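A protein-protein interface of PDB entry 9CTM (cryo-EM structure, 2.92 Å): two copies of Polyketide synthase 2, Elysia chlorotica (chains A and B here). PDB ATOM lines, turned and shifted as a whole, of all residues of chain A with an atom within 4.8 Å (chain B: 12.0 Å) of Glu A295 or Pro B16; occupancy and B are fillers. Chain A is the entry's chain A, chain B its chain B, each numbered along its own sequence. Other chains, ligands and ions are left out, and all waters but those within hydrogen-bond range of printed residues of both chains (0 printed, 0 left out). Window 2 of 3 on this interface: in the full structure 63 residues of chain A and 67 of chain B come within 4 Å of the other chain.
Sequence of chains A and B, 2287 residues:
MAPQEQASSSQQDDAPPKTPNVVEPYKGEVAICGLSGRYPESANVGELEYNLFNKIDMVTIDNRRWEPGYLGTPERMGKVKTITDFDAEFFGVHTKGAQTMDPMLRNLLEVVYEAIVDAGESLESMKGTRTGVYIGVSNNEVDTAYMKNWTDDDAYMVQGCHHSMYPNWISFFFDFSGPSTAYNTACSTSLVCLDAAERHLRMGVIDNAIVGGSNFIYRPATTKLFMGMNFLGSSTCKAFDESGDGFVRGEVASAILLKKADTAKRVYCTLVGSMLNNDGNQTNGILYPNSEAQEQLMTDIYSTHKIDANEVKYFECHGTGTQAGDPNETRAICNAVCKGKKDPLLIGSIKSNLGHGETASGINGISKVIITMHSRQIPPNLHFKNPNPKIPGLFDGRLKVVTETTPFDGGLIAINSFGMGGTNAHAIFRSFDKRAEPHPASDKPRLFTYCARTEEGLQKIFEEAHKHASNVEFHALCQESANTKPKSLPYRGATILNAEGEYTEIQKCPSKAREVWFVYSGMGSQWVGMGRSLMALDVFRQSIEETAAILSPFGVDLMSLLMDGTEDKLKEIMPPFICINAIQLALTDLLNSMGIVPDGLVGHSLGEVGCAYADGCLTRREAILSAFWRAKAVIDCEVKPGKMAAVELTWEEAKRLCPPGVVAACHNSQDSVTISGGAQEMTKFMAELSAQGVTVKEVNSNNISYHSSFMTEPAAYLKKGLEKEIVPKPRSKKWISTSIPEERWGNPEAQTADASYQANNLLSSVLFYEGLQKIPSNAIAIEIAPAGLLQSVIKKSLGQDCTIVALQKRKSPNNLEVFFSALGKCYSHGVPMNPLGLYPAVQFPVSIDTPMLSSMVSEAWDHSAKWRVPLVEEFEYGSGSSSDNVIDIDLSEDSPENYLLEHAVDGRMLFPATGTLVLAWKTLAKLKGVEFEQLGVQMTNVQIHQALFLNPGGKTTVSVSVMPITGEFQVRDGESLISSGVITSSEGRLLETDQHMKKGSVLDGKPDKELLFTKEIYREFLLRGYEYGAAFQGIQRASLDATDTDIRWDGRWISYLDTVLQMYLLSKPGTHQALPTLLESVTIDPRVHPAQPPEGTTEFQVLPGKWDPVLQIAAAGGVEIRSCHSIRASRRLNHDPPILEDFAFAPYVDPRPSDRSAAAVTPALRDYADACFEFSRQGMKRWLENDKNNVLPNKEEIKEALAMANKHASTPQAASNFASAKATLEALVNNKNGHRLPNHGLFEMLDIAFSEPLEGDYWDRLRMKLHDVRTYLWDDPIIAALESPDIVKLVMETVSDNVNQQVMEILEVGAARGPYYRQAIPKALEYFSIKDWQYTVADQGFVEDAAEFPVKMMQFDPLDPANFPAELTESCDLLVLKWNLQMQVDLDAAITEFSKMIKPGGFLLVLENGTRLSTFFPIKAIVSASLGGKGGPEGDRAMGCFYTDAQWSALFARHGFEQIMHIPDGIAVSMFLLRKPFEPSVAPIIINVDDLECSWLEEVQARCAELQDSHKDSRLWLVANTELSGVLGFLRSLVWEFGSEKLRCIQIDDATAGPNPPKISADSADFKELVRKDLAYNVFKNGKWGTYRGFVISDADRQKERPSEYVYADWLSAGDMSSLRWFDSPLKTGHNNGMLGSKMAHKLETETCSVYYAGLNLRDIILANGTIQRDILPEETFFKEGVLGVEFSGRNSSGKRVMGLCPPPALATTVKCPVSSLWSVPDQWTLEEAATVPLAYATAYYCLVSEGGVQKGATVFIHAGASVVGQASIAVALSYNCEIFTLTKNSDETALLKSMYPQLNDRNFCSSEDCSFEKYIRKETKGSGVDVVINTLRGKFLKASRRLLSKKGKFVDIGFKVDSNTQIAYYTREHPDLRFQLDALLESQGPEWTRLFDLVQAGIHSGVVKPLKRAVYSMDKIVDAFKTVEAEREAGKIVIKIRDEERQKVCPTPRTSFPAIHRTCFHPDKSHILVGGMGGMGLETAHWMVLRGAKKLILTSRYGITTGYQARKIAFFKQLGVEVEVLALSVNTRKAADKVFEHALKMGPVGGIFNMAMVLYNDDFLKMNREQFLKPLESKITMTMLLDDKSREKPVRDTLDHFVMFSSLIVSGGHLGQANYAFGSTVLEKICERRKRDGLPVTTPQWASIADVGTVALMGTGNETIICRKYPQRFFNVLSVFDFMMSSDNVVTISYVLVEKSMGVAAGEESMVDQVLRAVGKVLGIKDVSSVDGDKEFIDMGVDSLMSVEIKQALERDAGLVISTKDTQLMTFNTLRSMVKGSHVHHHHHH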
ATOM      1  N   SER A 291     -25.199 -23.811 -25.436  1.00  0.00           N
ATOM      2  CA  SER A 291     -24.270 -22.718 -25.166  1.00  0.00           C
ATOM      3  C   SER A 291     -25.009 -21.463 -24.721  1.00  0.00           C
ATOM      4  O   SER A 291     -24.534 -20.728 -23.848  1.00  0.00           O
ATOM      5  CB  SER A 291     -23.426 -22.429 -26.407  1.00  0.00           C
ATOM      6  OG  SER A 291     -22.465 -21.422 -26.146  1.00  0.00           O
ATOM      7  N   GLU A 292     -26.173 -21.197 -25.318  1.00  0.00           N
ATOM      8  CA  GLU A 292     -26.919 -19.989 -24.979  1.00  0.00           C
ATOM      9  C   GLU A 292     -27.334 -19.993 -23.512  1.00  0.00           C
ATOM     10  O   GLU A 292     -27.206 -18.976 -22.819  1.00  0.00           O
ATOM     11  CB  GLU A 292     -28.148 -19.865 -25.881  1.00  0.00           C
ATOM     12  CG  GLU A 292     -27.832 -19.856 -27.372  1.00  0.00           C
ATOM     13  CD  GLU A 292     -27.292 -18.524 -27.855  1.00  0.00           C
ATOM     14  OE1 GLU A 292     -27.616 -17.488 -27.238  1.00  0.00           O
ATOM     15  OE2 GLU A 292     -26.541 -18.514 -28.853  1.00  0.00           O
ATOM     16  N   ALA A 293     -27.836 -21.129 -23.022  1.00  0.00           N
ATOM     17  CA  ALA A 293     -28.258 -21.210 -21.627  1.00  0.00           C
ATOM     18  C   ALA A 293     -27.081 -21.021 -20.680  1.00  0.00           C
ATOM     19  O   ALA A 293     -27.199 -20.332 -19.659  1.00  0.00           O
ATOM     20  CB  ALA A 293     -28.944 -22.549 -21.366  1.00  0.00           C
ATOM     21  N   GLN A 294     -25.939 -21.636 -20.993  1.00  0.00           N
ATOM     22  CA  GLN A 294     -24.758 -21.479 -20.149  1.00  0.00           C
ATOM     23  C   GLN A 294     -24.291 -20.028 -20.124  1.00  0.00           C
ATOM     24  O   GLN A 294     -23.939 -19.494 -19.064  1.00  0.00           O
ATOM     25  CB  GLN A 294     -23.641 -22.392 -20.648  1.00  0.00           C
ATOM     26  CG  GLN A 294     -24.016 -23.868 -20.691  1.00  0.00           C
ATOM     27  CD  GLN A 294     -23.121 -24.671 -21.615  1.00  0.00           C
ATOM     28  OE1 GLN A 294     -22.151 -24.152 -22.166  1.00  0.00           O
ATOM     29  NE2 GLN A 294     -23.446 -25.948 -21.789  1.00  0.00           N
ATOM     30  N   GLU A 295     -24.278 -19.378 -21.291  1.00  0.00           N
ATOM     31  CA  GLU A 295     -23.896 -17.972 -21.348  1.00  0.00           C
ATOM     32  C   GLU A 295     -24.850 -17.116 -20.528  1.00  0.00           C
ATOM     33  O   GLU A 295     -24.418 -16.208 -19.808  1.00  0.00           O
ATOM     34  CB  GLU A 295     -23.865 -17.502 -22.802  1.00  0.00           C
ATOM     35  CG  GLU A 295     -23.358 -16.083 -22.990  1.00  0.00           C
ATOM     36  CD  GLU A 295     -23.393 -15.645 -24.441  1.00  0.00           C
ATOM     37  OE1 GLU A 295     -23.319 -16.519 -25.330  1.00  0.00           O
ATOM     38  OE2 GLU A 295     -23.493 -14.425 -24.693  1.00  0.00           O
ATOM     39  N   GLN A 296     -26.153 -17.388 -20.627  1.00  0.00           N
ATOM     40  CA  GLN A 296     -27.125 -16.635 -19.841  1.00  0.00           C
ATOM     41  C   GLN A 296     -26.905 -16.845 -18.349  1.00  0.00           C
ATOM     42  O   GLN A 296     -26.987 -15.895 -17.562  1.00  0.00           O
ATOM     43  CB  GLN A 296     -28.545 -17.043 -20.240  1.00  0.00           C
ATOM     44  CG  GLN A 296     -29.657 -16.361 -19.447  1.00  0.00           C
ATOM     45  CD  GLN A 296     -29.818 -14.894 -19.795  1.00  0.00           C
ATOM     46  OE1 GLN A 296     -28.896 -14.258 -20.305  1.00  0.00           O
ATOM     47  NE2 GLN A 296     -30.996 -14.348 -19.518  1.00  0.00           N
ATOM     48  N   LEU A 297     -26.631 -18.084 -17.938  1.00  0.00           N
ATOM     49  CA  LEU A 297     -26.386 -18.364 -16.526  1.00  0.00           C
ATOM     50  C   LEU A 297     -25.170 -17.596 -16.021  1.00  0.00           C
ATOM     51  O   LEU A 297     -25.205 -16.982 -14.945  1.00  0.00           O
ATOM     52  CB  LEU A 297     -26.194 -19.870 -16.326  1.00  0.00           C
ATOM     53  CG  LEU A 297     -25.552 -20.326 -15.014  1.00  0.00           C
ATOM     54  CD1 LEU A 297     -26.366 -19.847 -13.825  1.00  0.00           C
ATOM     55  CD2 LEU A 297     -25.399 -21.840 -14.990  1.00  0.00           C
ATOM     56  N   MET A 298     -24.077 -17.631 -16.788  1.00  0.00           N
ATOM     57  CA  MET A 298     -22.867 -16.928 -16.372  1.00  0.00           C
ATOM     58  C   MET A 298     -23.095 -15.422 -16.330  1.00  0.00           C
ATOM     59  O   MET A 298     -22.635 -14.741 -15.405  1.00  0.00           O
ATOM     60  CB  MET A 298     -21.708 -17.284 -17.302  1.00  0.00           C
ATOM     61  CG  MET A 298     -20.994 -18.575 -16.899  1.00  0.00           C
ATOM     62  SD  MET A 298     -19.710 -19.171 -18.023  1.00  0.00           S
ATOM     63  CE  MET A 298     -20.249 -18.515 -19.596  1.00  0.00           C
ATOM     64  N   THR A 299     -23.814 -14.882 -17.316  1.00  0.00           N
ATOM     65  CA  THR A 299     -24.126 -13.458 -17.301  1.00  0.00           C
ATOM     66  C   THR A 299     -24.953 -13.097 -16.074  1.00  0.00           C
ATOM     67  O   THR A 299     -24.696 -12.081 -15.420  1.00  0.00           O
ATOM     68  CB  THR A 299     -24.868 -13.075 -18.581  1.00  0.00           C
ATOM     69  OG1 THR A 299     -24.008 -13.266 -19.710  1.00  0.00           O
ATOM     70  CG2 THR A 299     -25.319 -11.624 -18.530  1.00  0.00           C
ATOM     71  N   ALA A 332     -19.457 -20.096 -24.705  1.00  0.00           N
ATOM     72  CA  ALA A 332     -20.099 -19.371 -23.613  1.00  0.00           C
ATOM     73  C   ALA A 332     -19.076 -18.581 -22.808  1.00  0.00           C
ATOM     74  O   ALA A 332     -19.304 -17.411 -22.473  1.00  0.00           O
ATOM     75  CB  ALA A 332     -20.856 -20.347 -22.713  1.00  0.00           C
ATOM     76  N   ASN A 335     -17.959 -15.543 -24.820  1.00  0.00           N
ATOM     77  CA  ASN A 335     -18.994 -14.532 -24.997  1.00  0.00           C
ATOM     78  C   ASN A 335     -19.315 -13.807 -23.696  1.00  0.00           C
ATOM     79  O   ASN A 335     -19.699 -12.634 -23.725  1.00  0.00           O
ATOM     80  CB  ASN A 335     -20.262 -15.172 -25.560  1.00  0.00           C
ATOM     81  CG  ASN A 335     -20.331 -15.097 -27.074  1.00  0.00           C
ATOM     82  OD1 ASN A 335     -19.557 -15.747 -27.775  1.00  0.00           O
ATOM     83  ND2 ASN A 335     -21.264 -14.301 -27.584  1.00  0.00           N
ATOM     84  N   ALA A 336     -19.173 -14.479 -22.553  1.00  0.00           N
ATOM     85  CA  ALA A 336     -19.592 -13.904 -21.281  1.00  0.00           C
ATOM     86  C   ALA A 336     -18.443 -13.382 -20.431  1.00  0.00           C
ATOM     87  O   ALA A 336     -18.612 -12.367 -19.747  1.00  0.00           O
ATOM     88  CB  ALA A 336     -20.373 -14.942 -20.472  1.00  0.00           C
ATOM     89  N   PRO B  16     -25.814 -10.030 -30.004  1.00  0.00           N
ATOM     90  CA  PRO B  16     -25.081 -11.134 -29.378  1.00  0.00           C
ATOM     91  C   PRO B  16     -25.016 -11.038 -27.850  1.00  0.00           C
ATOM     92  O   PRO B  16     -25.187 -12.061 -27.186  1.00  0.00           O
ATOM     93  CB  PRO B  16     -23.676 -11.028 -29.995  1.00  0.00           C
ATOM     94  CG  PRO B  16     -23.762  -9.973 -31.086  1.00  0.00           C
ATOM     95  CD  PRO B  16     -25.199  -9.616 -31.274  1.00  0.00           C
ATOM     96  N   PRO B  17     -24.774  -9.847 -27.300  1.00  0.00           N
ATOM     97  CA  PRO B  17     -24.777  -9.712 -25.838  1.00  0.00           C
ATOM     98  C   PRO B  17     -26.122 -10.117 -25.251  1.00  0.00           C
ATOM     99  O   PRO B  17     -27.176  -9.883 -25.843  1.00  0.00           O
ATOM    100  CB  PRO B  17     -24.488  -8.223 -25.613  1.00  0.00           C
ATOM    101  CG  PRO B  17     -23.799  -7.776 -26.845  1.00  0.00           C
ATOM    102  CD  PRO B  17     -24.369  -8.594 -27.963  1.00  0.00           C
ATOM    103  N   LYS B  18     -26.071 -10.731 -24.072  1.00  0.00           N
ATOM    104  CA  LYS B  18     -27.261 -11.220 -23.387  1.00  0.00           C
ATOM    105  C   LYS B  18     -27.621 -10.276 -22.248  1.00  0.00           C
ATOM    106  O   LYS B  18     -26.754  -9.889 -21.457  1.00  0.00           O
ATOM    107  CB  LYS B  18     -27.035 -12.633 -22.849  1.00  0.00           C
ATOM    108  CG  LYS B  18     -27.118 -13.718 -23.914  1.00  0.00           C
ATOM    109  CD  LYS B  18     -27.560 -15.055 -23.335  1.00  0.00           C
ATOM    110  CE  LYS B  18     -28.371 -15.855 -24.342  1.00  0.00           C
ATOM    111  NZ  LYS B  18     -27.734 -15.894 -25.687  1.00  0.00           N
ATOM    112  N   THR B  19     -28.893  -9.910 -22.169  1.00  0.00           N
ATOM    113  CA  THR B  19     -29.359  -9.030 -21.105  1.00  0.00           C
ATOM    114  C   THR B  19     -29.441  -9.809 -19.797  1.00  0.00           C
ATOM    115  O   THR B  19     -30.169 -10.808 -19.731  1.00  0.00           O
ATOM    116  CB  THR B  19     -30.724  -8.446 -21.459  1.00  0.00           C
ATOM    117  OG1 THR B  19     -30.692  -7.919 -22.791  1.00  0.00           O
ATOM    118  CG2 THR B  19     -31.102  -7.337 -20.485  1.00  0.00           C
ATOM    119  N   PRO B  20     -28.726  -9.408 -18.745  1.00  0.00           N
ATOM    120  CA  PRO B  20     -28.812 -10.151 -17.481  1.00  0.00           C
ATOM    121  C   PRO B  20     -30.229 -10.144 -16.926  1.00  0.00           C
ATOM    122  O   PRO B  20     -30.954  -9.154 -17.030  1.00  0.00           O
ATOM    123  CB  PRO B  20     -27.843  -9.404 -16.557  1.00  0.00           C
ATOM    124  CG  PRO B  20     -26.946  -8.637 -17.458  1.00  0.00           C
ATOM    125  CD  PRO B  20     -27.742  -8.313 -18.678  1.00  0.00           C
ATOM    126  N   ASN B  21     -30.617 -11.269 -16.328  1.00  0.00           N
ATOM    127  CA  ASN B  21     -31.903 -11.360 -15.654  1.00  0.00           C
ATOM    128  C   ASN B  21     -31.838 -10.645 -14.311  1.00  0.00           C
ATOM    129  O   ASN B  21     -30.810 -10.666 -13.628  1.00  0.00           O
ATOM    130  CB  ASN B  21     -32.302 -12.822 -15.451  1.00  0.00           C
ATOM    131  CG  ASN B  21     -33.078 -13.386 -16.627  1.00  0.00           C
ATOM    132  OD1 ASN B  21     -33.822 -12.670 -17.298  1.00  0.00           O
ATOM    133  ND2 ASN B  21     -32.908 -14.678 -16.882  1.00  0.00           N
ATOM    134  N   VAL B  23     -32.343 -10.612 -10.798  1.00  0.00           N
ATOM    135  CA  VAL B  23     -32.510 -11.513  -9.663  1.00  0.00           C
ATOM    136  C   VAL B  23     -32.610 -10.640  -8.418  1.00  0.00           C
ATOM    137  O   VAL B  23     -31.600 -10.149  -7.905  1.00  0.00           O
ATOM    138  CB  VAL B  23     -31.359 -12.518  -9.562  1.00  0.00           C
ATOM    139  CG1 VAL B  23     -31.381 -13.222  -8.211  1.00  0.00           C
ATOM    140  CG2 VAL B  23     -31.434 -13.528 -10.696  1.00  0.00           C
ATOM    141  N   SER B 177     -36.686 -22.920 -17.733  1.00  0.00           N
ATOM    142  CA  SER B 177     -35.310 -22.444 -17.635  1.00  0.00           C
ATOM    143  C   SER B 177     -34.970 -22.106 -16.190  1.00  0.00           C
ATOM    144  O   SER B 177     -34.396 -21.059 -15.883  1.00  0.00           O
ATOM    145  CB  SER B 177     -35.091 -21.233 -18.538  1.00  0.00           C
ATOM    146  OG  SER B 177     -35.464 -20.034 -17.881  1.00  0.00           O
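Among the printed residues, merely in contact across the chains: Glu A295 with Pro B16, Glu A295 with Lys B18, Gln A296 with Lys B18, Gln A296 with Thr B19, Thr A299 with Lys B18 and Thr A299 with Pro B20.
No position is printed for both chains.
Of the 8 pairs that touch across the chains among the printed residues, none has its exchanged pair printed and touching as well.
Of the 8 printed residues of chain B, 5 touch a printed residue of chain A.
Printed residues of chain B that touch a printed residue of chain A: Pro B16, Lys B18, Thr B19, Pro B20 and Asn B21.
Hydrophobic or aromatic side chains of chain B within 4 Å of the printed part of chain A: Pro B20.
Of the 12 printed residues of chain A, 4 touch a printed residue of chain B.
Among the printed residues, Asp or Glu carboxylates within 4 Å of a Lys or Arg side-chain nitrogen of the other chain: Glu A292 with Lys B18.
The side-chain amide nitrogen (NE2) of Gln A296 sits close to the side-chain amide nitrogen (ND2) of Asn B21 (3.3 Å).
OE1 of Glu A292 lies close to NZ of Lys B18, 2.2 Å away.
No residue of chain B comes within 4 Å of Ser A291.
No residue of chain B comes within 4 Å of Ala A293.
No residue of chain B comes within 4 Å of Gln A294.
No residue of chain B comes within 4 Å of Leu A297.
No residue of chain B comes within 4 Å of Met A298.
Ala A332 touches none of the printed residues of chain B.
Pro B17 touches none of the printed residues of chain A.
Printed residues of chain A within 4 Å of Lys B18: Glu A292, Glu A295, Gln A296 and Thr A299.
Of the printed residues of chain A, Thr B19 touches Gln A296.
Of the printed residues of chain A, Pro B20 touches Thr A299.
Of the printed residues of chain A, Asn B21 touches Gln A296 (3.3 Å).
Ser B177 touches none of the printed residues of chain A.
The nearest residue of chain B that does not touch Glu A295 is Pro B17 (5.0 Å).
The nearest residue of chain A that does not touch Pro B16 is Asn A335 (4.5 Å).
OG1 of Thr A299 is in hydrogen-bond range of O of Glu A295 (3.0 Å).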
